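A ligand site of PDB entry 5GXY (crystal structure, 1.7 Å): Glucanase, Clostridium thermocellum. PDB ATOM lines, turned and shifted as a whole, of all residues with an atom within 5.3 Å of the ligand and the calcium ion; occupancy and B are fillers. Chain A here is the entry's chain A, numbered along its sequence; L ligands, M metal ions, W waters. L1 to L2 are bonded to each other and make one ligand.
Merely in contact with the ligand: His 194 and Trp 245.
The side-chain sulfur of Cys 244 lies close to the backbone NH of Asp 246.
The side-chain carboxylate of Asp 246 sits at hydrogen-bond distance from the backbone NH of His 194 (2.9 Å).
OD1 of Asn 229 lies close to O of Ser 195 (2.9 Å).
The backbone NH (N) of Glu 238 sits at hydrogen-bond distance from the backbone carbonyl oxygen (O) of Asn 229 (2.9 Å).
N of Trp 241 sits close to OH of Tyr 250 (3.5 Å).
Of the 20 residues printed, 5 come within 4 Å of the calcium ion.
The calcium ion is bound by the side-chain carboxylate (OE2) of Glu 200, the backbone carbonyl oxygen (O) of Asp 246, the backbone carbonyl oxygen (O) of Gly 196, the side-chain carboxylate (OD2) of Asp 199, water W2, the side-chain hydroxyl (OG) of Ser 195, the side-chain carboxylate (OE1) of Glu 200 and the side-chain carboxylate (OD1) of Asp 199.
The calcium ion has eight donor atoms within binding distance.
Water W2 bridges the side-chain carboxylate of Asp 246 and the side-chain hydroxyl of Ser 193.
Water W3 lies within hydrogen-bond range of O5 of LIG L1 (2.9 Å), NE1 of Trp 245 (3.0 Å) and OH of Tyr 304 (3.2 Å).
Water W4 bridges an oxygen (O2) of LG2 L2 (2.9 Å) and the side-chain amide oxygen (OD1) of Asn 229 (3.4 Å).
Water W1 lies within hydrogen-bond range of OD2 of Asp 297 (2.5 Å), OH of Tyr 304 (2.7 Å) and O1 of LIG L1 (3.0 Å).
OD2 of Asp 246 sits at hydrogen-bond distance from O1 of LG2 L2 (2.5 Å).
The side-chain carboxylate (OE1) of Glu 238 is in hydrogen-bond range of an oxygen (O3) of LG2 L2, at 2.7 Å.
The side-chain hydroxyl (OH) of Tyr 304 lies within hydrogen-bond range of an oxygen (O6) of LIG L1.
NE1 of Trp 241 sits at hydrogen-bond distance from O6 of LIG L1 (2.9 Å).
OD2 of Asp 247 sits at hydrogen-bond distance from O2 of LG2 L2, 3.1 Å away.
The side-chain sulfur of Cys 244 lies within hydrogen-bond range of an oxygen (O6) of LIG L1.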
ATOM      1  N   ALA A 143      29.815  -7.882  -5.642  1.00  0.00           N
ATOM      2  CA  ALA A 143      28.689  -7.481  -6.510  1.00  0.00           C
ATOM      3  C   ALA A 143      27.328  -7.996  -6.035  1.00  0.00           C
ATOM      4  O   ALA A 143      26.388  -7.214  -5.856  1.00  0.00           O
ATOM      5  CB  ALA A 143      28.938  -7.842  -7.982  1.00  0.00           C
ATOM      6  N   SER A 193      29.628 -11.733 -13.157  1.00  0.00           N
ATOM      7  CA  SER A 193      29.933 -10.340 -12.877  1.00  0.00           C
ATOM      8  C   SER A 193      30.857  -9.825 -13.981  1.00  0.00           C
ATOM      9  O   SER A 193      32.045 -10.168 -14.049  1.00  0.00           O
ATOM     10  CB  SER A 193      30.564 -10.170 -11.481  1.00  0.00           C
ATOM     11  OG  SER A 193      30.923  -8.809 -11.277  1.00  0.00           O
ATOM     12  N   HIS A 194      30.282  -9.020 -14.873  1.00  0.00           N
ATOM     13  CA  HIS A 194      31.002  -8.524 -16.048  1.00  0.00           C
ATOM     14  C   HIS A 194      31.761  -7.230 -15.745  1.00  0.00           C
ATOM     15  O   HIS A 194      32.909  -7.068 -16.168  1.00  0.00           O
ATOM     16  CB  HIS A 194      30.027  -8.282 -17.202  1.00  0.00           C
ATOM     17  CG  HIS A 194      29.332  -9.520 -17.678  1.00  0.00           C
ATOM     18  ND1 HIS A 194      29.897 -10.370 -18.602  1.00  0.00           N
ATOM     19  CD2 HIS A 194      28.132 -10.049 -17.348  1.00  0.00           C
ATOM     20  CE1 HIS A 194      29.066 -11.376 -18.829  1.00  0.00           C
ATOM     21  NE2 HIS A 194      27.985 -11.200 -18.084  1.00  0.00           N
ATOM     22  N   SER A 195      31.124  -6.325 -15.025  1.00  0.00           N
ATOM     23  CA  SER A 195      31.665  -4.976 -14.822  1.00  0.00           C
ATOM     24  C   SER A 195      32.512  -4.924 -13.559  1.00  0.00           C
ATOM     25  O   SER A 195      33.145  -3.913 -13.283  1.00  0.00           O
ATOM     26  CB  SER A 195      30.515  -3.967 -14.690  1.00  0.00           C
ATOM     27  OG  SER A 195      29.535  -4.429 -13.755  1.00  0.00           O
ATOM     28  N   GLY A 196      32.530  -6.016 -12.788  1.00  0.00           N
ATOM     29  CA  GLY A 196      33.141  -5.987 -11.458  1.00  0.00           C
ATOM     30  C   GLY A 196      32.206  -5.414 -10.409  1.00  0.00           C
ATOM     31  O   GLY A 196      31.006  -5.267 -10.658  1.00  0.00           O
ATOM     32  N   PHE A 197      32.746  -5.086  -9.231  1.00  0.00           N
ATOM     33  CA  PHE A 197      31.899  -4.797  -8.067  1.00  0.00           C
ATOM     34  C   PHE A 197      31.892  -3.334  -7.631  1.00  0.00           C
ATOM     35  O   PHE A 197      31.132  -2.975  -6.724  1.00  0.00           O
ATOM     36  CB  PHE A 197      32.300  -5.671  -6.870  1.00  0.00           C
ATOM     37  CG  PHE A 197      33.725  -5.458  -6.435  1.00  0.00           C
ATOM     38  CD1 PHE A 197      34.076  -4.318  -5.737  1.00  0.00           C
ATOM     39  CD2 PHE A 197      34.707  -6.356  -6.815  1.00  0.00           C
ATOM     40  CE1 PHE A 197      35.399  -4.067  -5.368  1.00  0.00           C
ATOM     41  CE2 PHE A 197      36.042  -6.111  -6.464  1.00  0.00           C
ATOM     42  CZ  PHE A 197      36.380  -4.967  -5.765  1.00  0.00           C
ATOM     43  N   ASP A 199      30.726  -0.660  -9.048  1.00  0.00           N
ATOM     44  CA  ASP A 199      29.410  -0.057  -9.282  1.00  0.00           C
ATOM     45  C   ASP A 199      28.376  -0.448  -8.228  1.00  0.00           C
ATOM     46  O   ASP A 199      27.567   0.382  -7.807  1.00  0.00           O
ATOM     47  CB  ASP A 199      28.903  -0.391 -10.694  1.00  0.00           C
ATOM     48  CG  ASP A 199      28.967  -1.881 -10.993  1.00  0.00           C
ATOM     49  OD1 ASP A 199      30.083  -2.393 -11.247  1.00  0.00           O
ATOM     50  OD2 ASP A 199      27.918  -2.570 -10.949  1.00  0.00           O
ATOM     51  N   GLU A 200      28.395  -1.698  -7.791  1.00  0.00           N
ATOM     52  CA  GLU A 200      27.502  -2.143  -6.707  1.00  0.00           C
ATOM     53  C   GLU A 200      27.814  -1.417  -5.401  1.00  0.00           C
ATOM     54  O   GLU A 200      26.894  -1.000  -4.692  1.00  0.00           O
ATOM     55  CB  GLU A 200      27.548  -3.660  -6.501  1.00  0.00           C
ATOM     56  CG  GLU A 200      26.836  -4.467  -7.601  1.00  0.00           C
ATOM     57  CD  GLU A 200      27.701  -4.715  -8.834  1.00  0.00           C
ATOM     58  OE1 GLU A 200      28.856  -4.227  -8.848  1.00  0.00           O
ATOM     59  OE2 GLU A 200      27.249  -5.364  -9.818  1.00  0.00           O
ATOM     60  N   ASN A 229      34.660   1.533 -14.312  1.00  0.00           N
ATOM     61  CA  ASN A 229      35.203   1.296 -15.650  1.00  0.00           C
ATOM     62  C   ASN A 229      35.138   2.551 -16.515  1.00  0.00           C
ATOM     63  O   ASN A 229      34.215   3.369 -16.381  1.00  0.00           O
ATOM     64  CB  ASN A 229      34.502   0.112 -16.340  1.00  0.00           C
ATOM     65  CG  ASN A 229      34.545  -1.158 -15.513  1.00  0.00           C
ATOM     66  OD1 ASN A 229      33.540  -1.864 -15.355  1.00  0.00           O
ATOM     67  ND2 ASN A 229      35.709  -1.454 -14.955  1.00  0.00           N
ATOM     68  N   GLU A 238      32.464   4.944 -18.017  1.00  0.00           N
ATOM     69  CA  GLU A 238      31.723   4.245 -19.055  1.00  0.00           C
ATOM     70  C   GLU A 238      30.274   4.734 -19.093  1.00  0.00           C
ATOM     71  O   GLU A 238      29.639   4.847 -18.050  1.00  0.00           O
ATOM     72  CB  GLU A 238      31.779   2.748 -18.794  1.00  0.00           C
ATOM     73  CG  GLU A 238      31.173   1.898 -19.891  1.00  0.00           C
ATOM     74  CD  GLU A 238      31.689   0.468 -19.834  1.00  0.00           C
ATOM     75  OE1 GLU A 238      31.230  -0.303 -18.961  1.00  0.00           O
ATOM     76  OE2 GLU A 238      32.571   0.128 -20.653  1.00  0.00           O
ATOM     77  N   GLN A 240      28.269   4.078 -22.321  1.00  0.00           N
ATOM     78  CA  GLN A 240      27.655   3.390 -23.457  1.00  0.00           C
ATOM     79  C   GLN A 240      27.107   2.003 -23.149  1.00  0.00           C
ATOM     80  O   GLN A 240      27.491   0.996 -23.759  1.00  0.00           O
ATOM     81  CB  GLN A 240      28.611   3.324 -24.663  1.00  0.00           C
ATOM     82  CG  GLN A 240      28.924   4.691 -25.230  1.00  0.00           C
ATOM     83  CD  GLN A 240      29.899   4.653 -26.400  1.00  0.00           C
ATOM     84  OE1 GLN A 240      30.132   3.594 -26.993  1.00  0.00           O
ATOM     85  NE2 GLN A 240      30.479   5.805 -26.739  1.00  0.00           N
ATOM     86  N   TRP A 241      26.178   1.959 -22.202  1.00  0.00           N
ATOM     87  CA  TRP A 241      25.450   0.741 -21.845  1.00  0.00           C
ATOM     88  C   TRP A 241      24.227   1.201 -21.065  1.00  0.00           C
ATOM     89  O   TRP A 241      23.958   2.398 -20.995  1.00  0.00           O
ATOM     90  CB  TRP A 241      26.347  -0.206 -21.033  1.00  0.00           C
ATOM     91  CG  TRP A 241      25.831  -1.614 -21.052  1.00  0.00           C
ATOM     92  CD1 TRP A 241      25.263  -2.307 -20.026  1.00  0.00           C
ATOM     93  CD2 TRP A 241      25.847  -2.495 -22.181  1.00  0.00           C
ATOM     94  NE1 TRP A 241      24.899  -3.565 -20.449  1.00  0.00           N
ATOM     95  CE2 TRP A 241      25.274  -3.705 -21.767  1.00  0.00           C
ATOM     96  CE3 TRP A 241      26.330  -2.380 -23.492  1.00  0.00           C
ATOM     97  CZ2 TRP A 241      25.120  -4.794 -22.619  1.00  0.00           C
ATOM     98  CZ3 TRP A 241      26.182  -3.453 -24.339  1.00  0.00           C
ATOM     99  CH2 TRP A 241      25.598  -4.655 -23.890  1.00  0.00           C
ATOM    100  N   CYS A 244      21.490  -1.841 -15.359  1.00  0.00           N
ATOM    101  CA  CYS A 244      21.023  -3.224 -15.471  1.00  0.00           C
ATOM    102  C   CYS A 244      21.514  -4.029 -14.276  1.00  0.00           C
ATOM    103  O   CYS A 244      22.296  -3.535 -13.459  1.00  0.00           O
ATOM    104  CB  CYS A 244      21.509  -3.883 -16.769  1.00  0.00           C
ATOM    105  SG  CYS A 244      23.325  -4.001 -16.848  1.00  0.00           S
ATOM    106  N   TRP A 245      21.067  -5.285 -14.216  1.00  0.00           N
ATOM    107  CA  TRP A 245      21.437  -6.212 -13.145  1.00  0.00           C
ATOM    108  C   TRP A 245      22.935  -6.300 -12.842  1.00  0.00           C
ATOM    109  O   TRP A 245      23.299  -6.584 -11.701  1.00  0.00           O
ATOM    110  CB  TRP A 245      20.884  -7.612 -13.406  1.00  0.00           C
ATOM    111  CG  TRP A 245      21.450  -8.241 -14.631  1.00  0.00           C
ATOM    112  CD1 TRP A 245      20.902  -8.244 -15.899  1.00  0.00           C
ATOM    113  CD2 TRP A 245      22.675  -8.984 -14.726  1.00  0.00           C
ATOM    114  NE1 TRP A 245      21.727  -8.927 -16.772  1.00  0.00           N
ATOM    115  CE2 TRP A 245      22.822  -9.377 -16.071  1.00  0.00           C
ATOM    116  CE3 TRP A 245      23.682  -9.326 -13.802  1.00  0.00           C
ATOM    117  CZ2 TRP A 245      23.928 -10.118 -16.529  1.00  0.00           C
ATOM    118  CZ3 TRP A 245      24.778 -10.053 -14.249  1.00  0.00           C
ATOM    119  CH2 TRP A 245      24.892 -10.433 -15.605  1.00  0.00           C
ATOM    120  N   ASP A 246      23.770  -6.107 -13.856  1.00  0.00           N
ATOM    121  CA  ASP A 246      25.225  -6.194 -13.701  1.00  0.00           C
ATOM    122  C   ASP A 246      25.915  -4.918 -13.275  1.00  0.00           C
ATOM    123  O   ASP A 246      27.060  -4.948 -12.783  1.00  0.00           O
ATOM    124  CB  ASP A 246      25.863  -6.663 -15.018  1.00  0.00           C
ATOM    125  CG  ASP A 246      27.352  -6.895 -14.857  1.00  0.00           C
ATOM    126  OD1 ASP A 246      27.682  -7.852 -14.129  1.00  0.00           O
ATOM    127  OD2 ASP A 246      28.143  -6.125 -15.448  1.00  0.00           O
ATOM    128  N   ASP A 247      25.260  -3.787 -13.530  1.00  0.00           N
ATOM    129  CA  ASP A 247      25.900  -2.481 -13.476  1.00  0.00           C
ATOM    130  C   ASP A 247      24.887  -1.363 -13.261  1.00  0.00           C
ATOM    131  O   ASP A 247      24.186  -0.935 -14.175  1.00  0.00           O
ATOM    132  CB  ASP A 247      26.663  -2.242 -14.791  1.00  0.00           C
ATOM    133  CG  ASP A 247      27.607  -1.058 -14.713  1.00  0.00           C
ATOM    134  OD1 ASP A 247      27.548  -0.263 -13.734  1.00  0.00           O
ATOM    135  OD2 ASP A 247      28.393  -0.907 -15.666  1.00  0.00           O
ATOM    136  N   TYR A 250      25.084   3.843 -13.567  1.00  0.00           N
ATOM    137  CA  TYR A 250      24.216   4.793 -14.248  1.00  0.00           C
ATOM    138  C   TYR A 250      23.188   5.464 -13.346  1.00  0.00           C
ATOM    139  O   TYR A 250      23.162   6.687 -13.216  1.00  0.00           O
ATOM    140  CB  TYR A 250      23.487   4.051 -15.387  1.00  0.00           C
ATOM    141  CG  TYR A 250      24.499   3.468 -16.319  1.00  0.00           C
ATOM    142  CD1 TYR A 250      25.157   4.300 -17.214  1.00  0.00           C
ATOM    143  CD2 TYR A 250      24.850   2.124 -16.282  1.00  0.00           C
ATOM    144  CE1 TYR A 250      26.116   3.815 -18.059  1.00  0.00           C
ATOM    145  CE2 TYR A 250      25.832   1.621 -17.138  1.00  0.00           C
ATOM    146  CZ  TYR A 250      26.454   2.498 -18.011  1.00  0.00           C
ATOM    147  OH  TYR A 250      27.409   2.149 -18.951  1.00  0.00           O
ATOM    148  N   ASP A 297      21.380  -4.645 -27.372  1.00  0.00           N
ATOM    149  CA  ASP A 297      21.977  -5.971 -27.477  1.00  0.00           C
ATOM    150  C   ASP A 297      20.893  -6.925 -27.922  1.00  0.00           C
ATOM    151  O   ASP A 297      19.711  -6.666 -27.748  1.00  0.00           O
ATOM    152  CB  ASP A 297      22.539  -6.427 -26.112  1.00  0.00           C
ATOM    153  CG  ASP A 297      23.416  -7.673 -26.223  1.00  0.00           C
ATOM    154  OD1 ASP A 297      24.346  -7.686 -27.066  1.00  0.00           O
ATOM    155  OD2 ASP A 297      23.150  -8.688 -25.550  1.00  0.00           O
ATOM    156  N   TRP A 299      20.072  -9.666 -26.557  1.00  0.00           N
ATOM    157  CA  TRP A 299      19.325 -10.175 -25.391  1.00  0.00           C
ATOM    158  C   TRP A 299      18.590  -9.077 -24.630  1.00  0.00           C
ATOM    159  O   TRP A 299      19.197  -8.064 -24.271  1.00  0.00           O
ATOM    160  CB  TRP A 299      20.321 -10.821 -24.436  1.00  0.00           C
ATOM    161  CG  TRP A 299      20.761 -12.173 -24.888  1.00  0.00           C
ATOM    162  CD1 TRP A 299      21.837 -12.469 -25.673  1.00  0.00           C
ATOM    163  CD2 TRP A 299      20.136 -13.415 -24.554  1.00  0.00           C
ATOM    164  NE1 TRP A 299      21.926 -13.835 -25.846  1.00  0.00           N
ATOM    165  CE2 TRP A 299      20.897 -14.430 -25.174  1.00  0.00           C
ATOM    166  CE3 TRP A 299      19.013 -13.768 -23.788  1.00  0.00           C
ATOM    167  CZ2 TRP A 299      20.560 -15.789 -25.054  1.00  0.00           C
ATOM    168  CZ3 TRP A 299      18.679 -15.119 -23.675  1.00  0.00           C
ATOM    169  CH2 TRP A 299      19.449 -16.105 -24.304  1.00  0.00           C
ATOM    170  N   TYR A 304      16.450  -3.328 -21.503  1.00  0.00           N
ATOM    171  CA  TYR A 304      17.398  -2.226 -21.376  1.00  0.00           C
ATOM    172  C   TYR A 304      16.747  -0.875 -21.694  1.00  0.00           C
ATOM    173  O   TYR A 304      16.990   0.099 -20.984  1.00  0.00           O
ATOM    174  CB  TYR A 304      18.598  -2.427 -22.291  1.00  0.00           C
ATOM    175  CG  TYR A 304      19.476  -3.615 -21.966  1.00  0.00           C
ATOM    176  CD1 TYR A 304      20.132  -3.728 -20.730  1.00  0.00           C
ATOM    177  CD2 TYR A 304      19.756  -4.573 -22.944  1.00  0.00           C
ATOM    178  CE1 TYR A 304      20.980  -4.797 -20.466  1.00  0.00           C
ATOM    179  CE2 TYR A 304      20.616  -5.647 -22.699  1.00  0.00           C
ATOM    180  CZ  TYR A 304      21.212  -5.744 -21.449  1.00  0.00           C
ATOM    181  OH  TYR A 304      22.067  -6.789 -21.188  1.00  0.00           O
HETATM  182  C1  LIG L   1      26.228  -9.395 -21.645  1.00  0.00           C
HETATM  183  C2  LIG L   1      27.309  -8.572 -20.936  1.00  0.00           C
HETATM  184  C3  LIG L   1      26.644  -7.476 -20.110  1.00  0.00           C
HETATM  185  C4  LIG L   1      25.544  -8.045 -19.208  1.00  0.00           C
HETATM  186  C5  LIG L   1      24.751  -6.983 -18.474  1.00  0.00           C
HETATM  187  C6  LIG L   1      25.229  -9.926 -20.626  1.00  0.00           C
HETATM  188  O1  LIG L   1      24.162 -10.599 -21.305  1.00  0.00           O
HETATM  189  O2  LIG L   1      26.807 -10.473 -22.373  1.00  0.00           O
HETATM  190  O3  LIG L   1      28.154  -7.954 -21.911  1.00  0.00           O
HETATM  191  O4  LIG L   1      27.601  -6.814 -19.283  1.00  0.00           O
HETATM  192  O5  LIG L   1      24.633  -8.795 -19.996  1.00  0.00           O
HETATM  193  O6  LIG L   1      24.064  -6.132 -19.397  1.00  0.00           O
HETATM  194  C1  LG2 L   2      28.417  -4.745 -18.451  1.00  0.00           C
HETATM  195  C2  LG2 L   2      28.834  -3.335 -18.850  1.00  0.00           C
HETATM  196  C3  LG2 L   2      29.649  -3.344 -20.144  1.00  0.00           C
HETATM  197  C4  LG2 L   2      28.925  -4.145 -21.226  1.00  0.00           C
HETATM  198  C5  LG2 L   2      29.677  -4.207 -22.551  1.00  0.00           C
HETATM  199  C6  LG2 L   2      27.762  -5.439 -19.636  1.00  0.00           C
HETATM  200  O1  LG2 L   2      27.517  -4.611 -17.349  1.00  0.00           O
HETATM  201  O2  LG2 L   2      29.604  -2.751 -17.791  1.00  0.00           O
HETATM  202  O3  LG2 L   2      29.835  -1.994 -20.589  1.00  0.00           O
HETATM  203  O4  LG2 L   2      28.687  -5.459 -20.728  1.00  0.00           O
HETATM  204  O5  LG2 L   2      30.868  -4.977 -22.355  1.00  0.00           O
HETATM  205 CA    CA M   1      28.862  -4.673 -11.341  1.00  0.00          CA
HETATM  206  O   HOH W   1      22.731  -8.566 -23.040  1.00  0.00           O
HETATM  207  O   HOH W   2      28.941  -6.958 -11.899  1.00  0.00           O
HETATM  208  O   HOH W   3      21.866  -9.569 -19.686  1.00  0.00           O
HETATM  209  O   HOH W   4      32.371  -3.622 -18.001  1.00  0.00           O
HETATM  210  O   HOH W   5      32.851  -3.230 -22.068  1.00  0.00           O
HETATM  211  O   HOH W   6      30.014 -10.593 -22.347  1.00  0.00           O
HETATM  212  O   HOH W   7      31.041  -0.323 -16.216  1.00  0.00           O
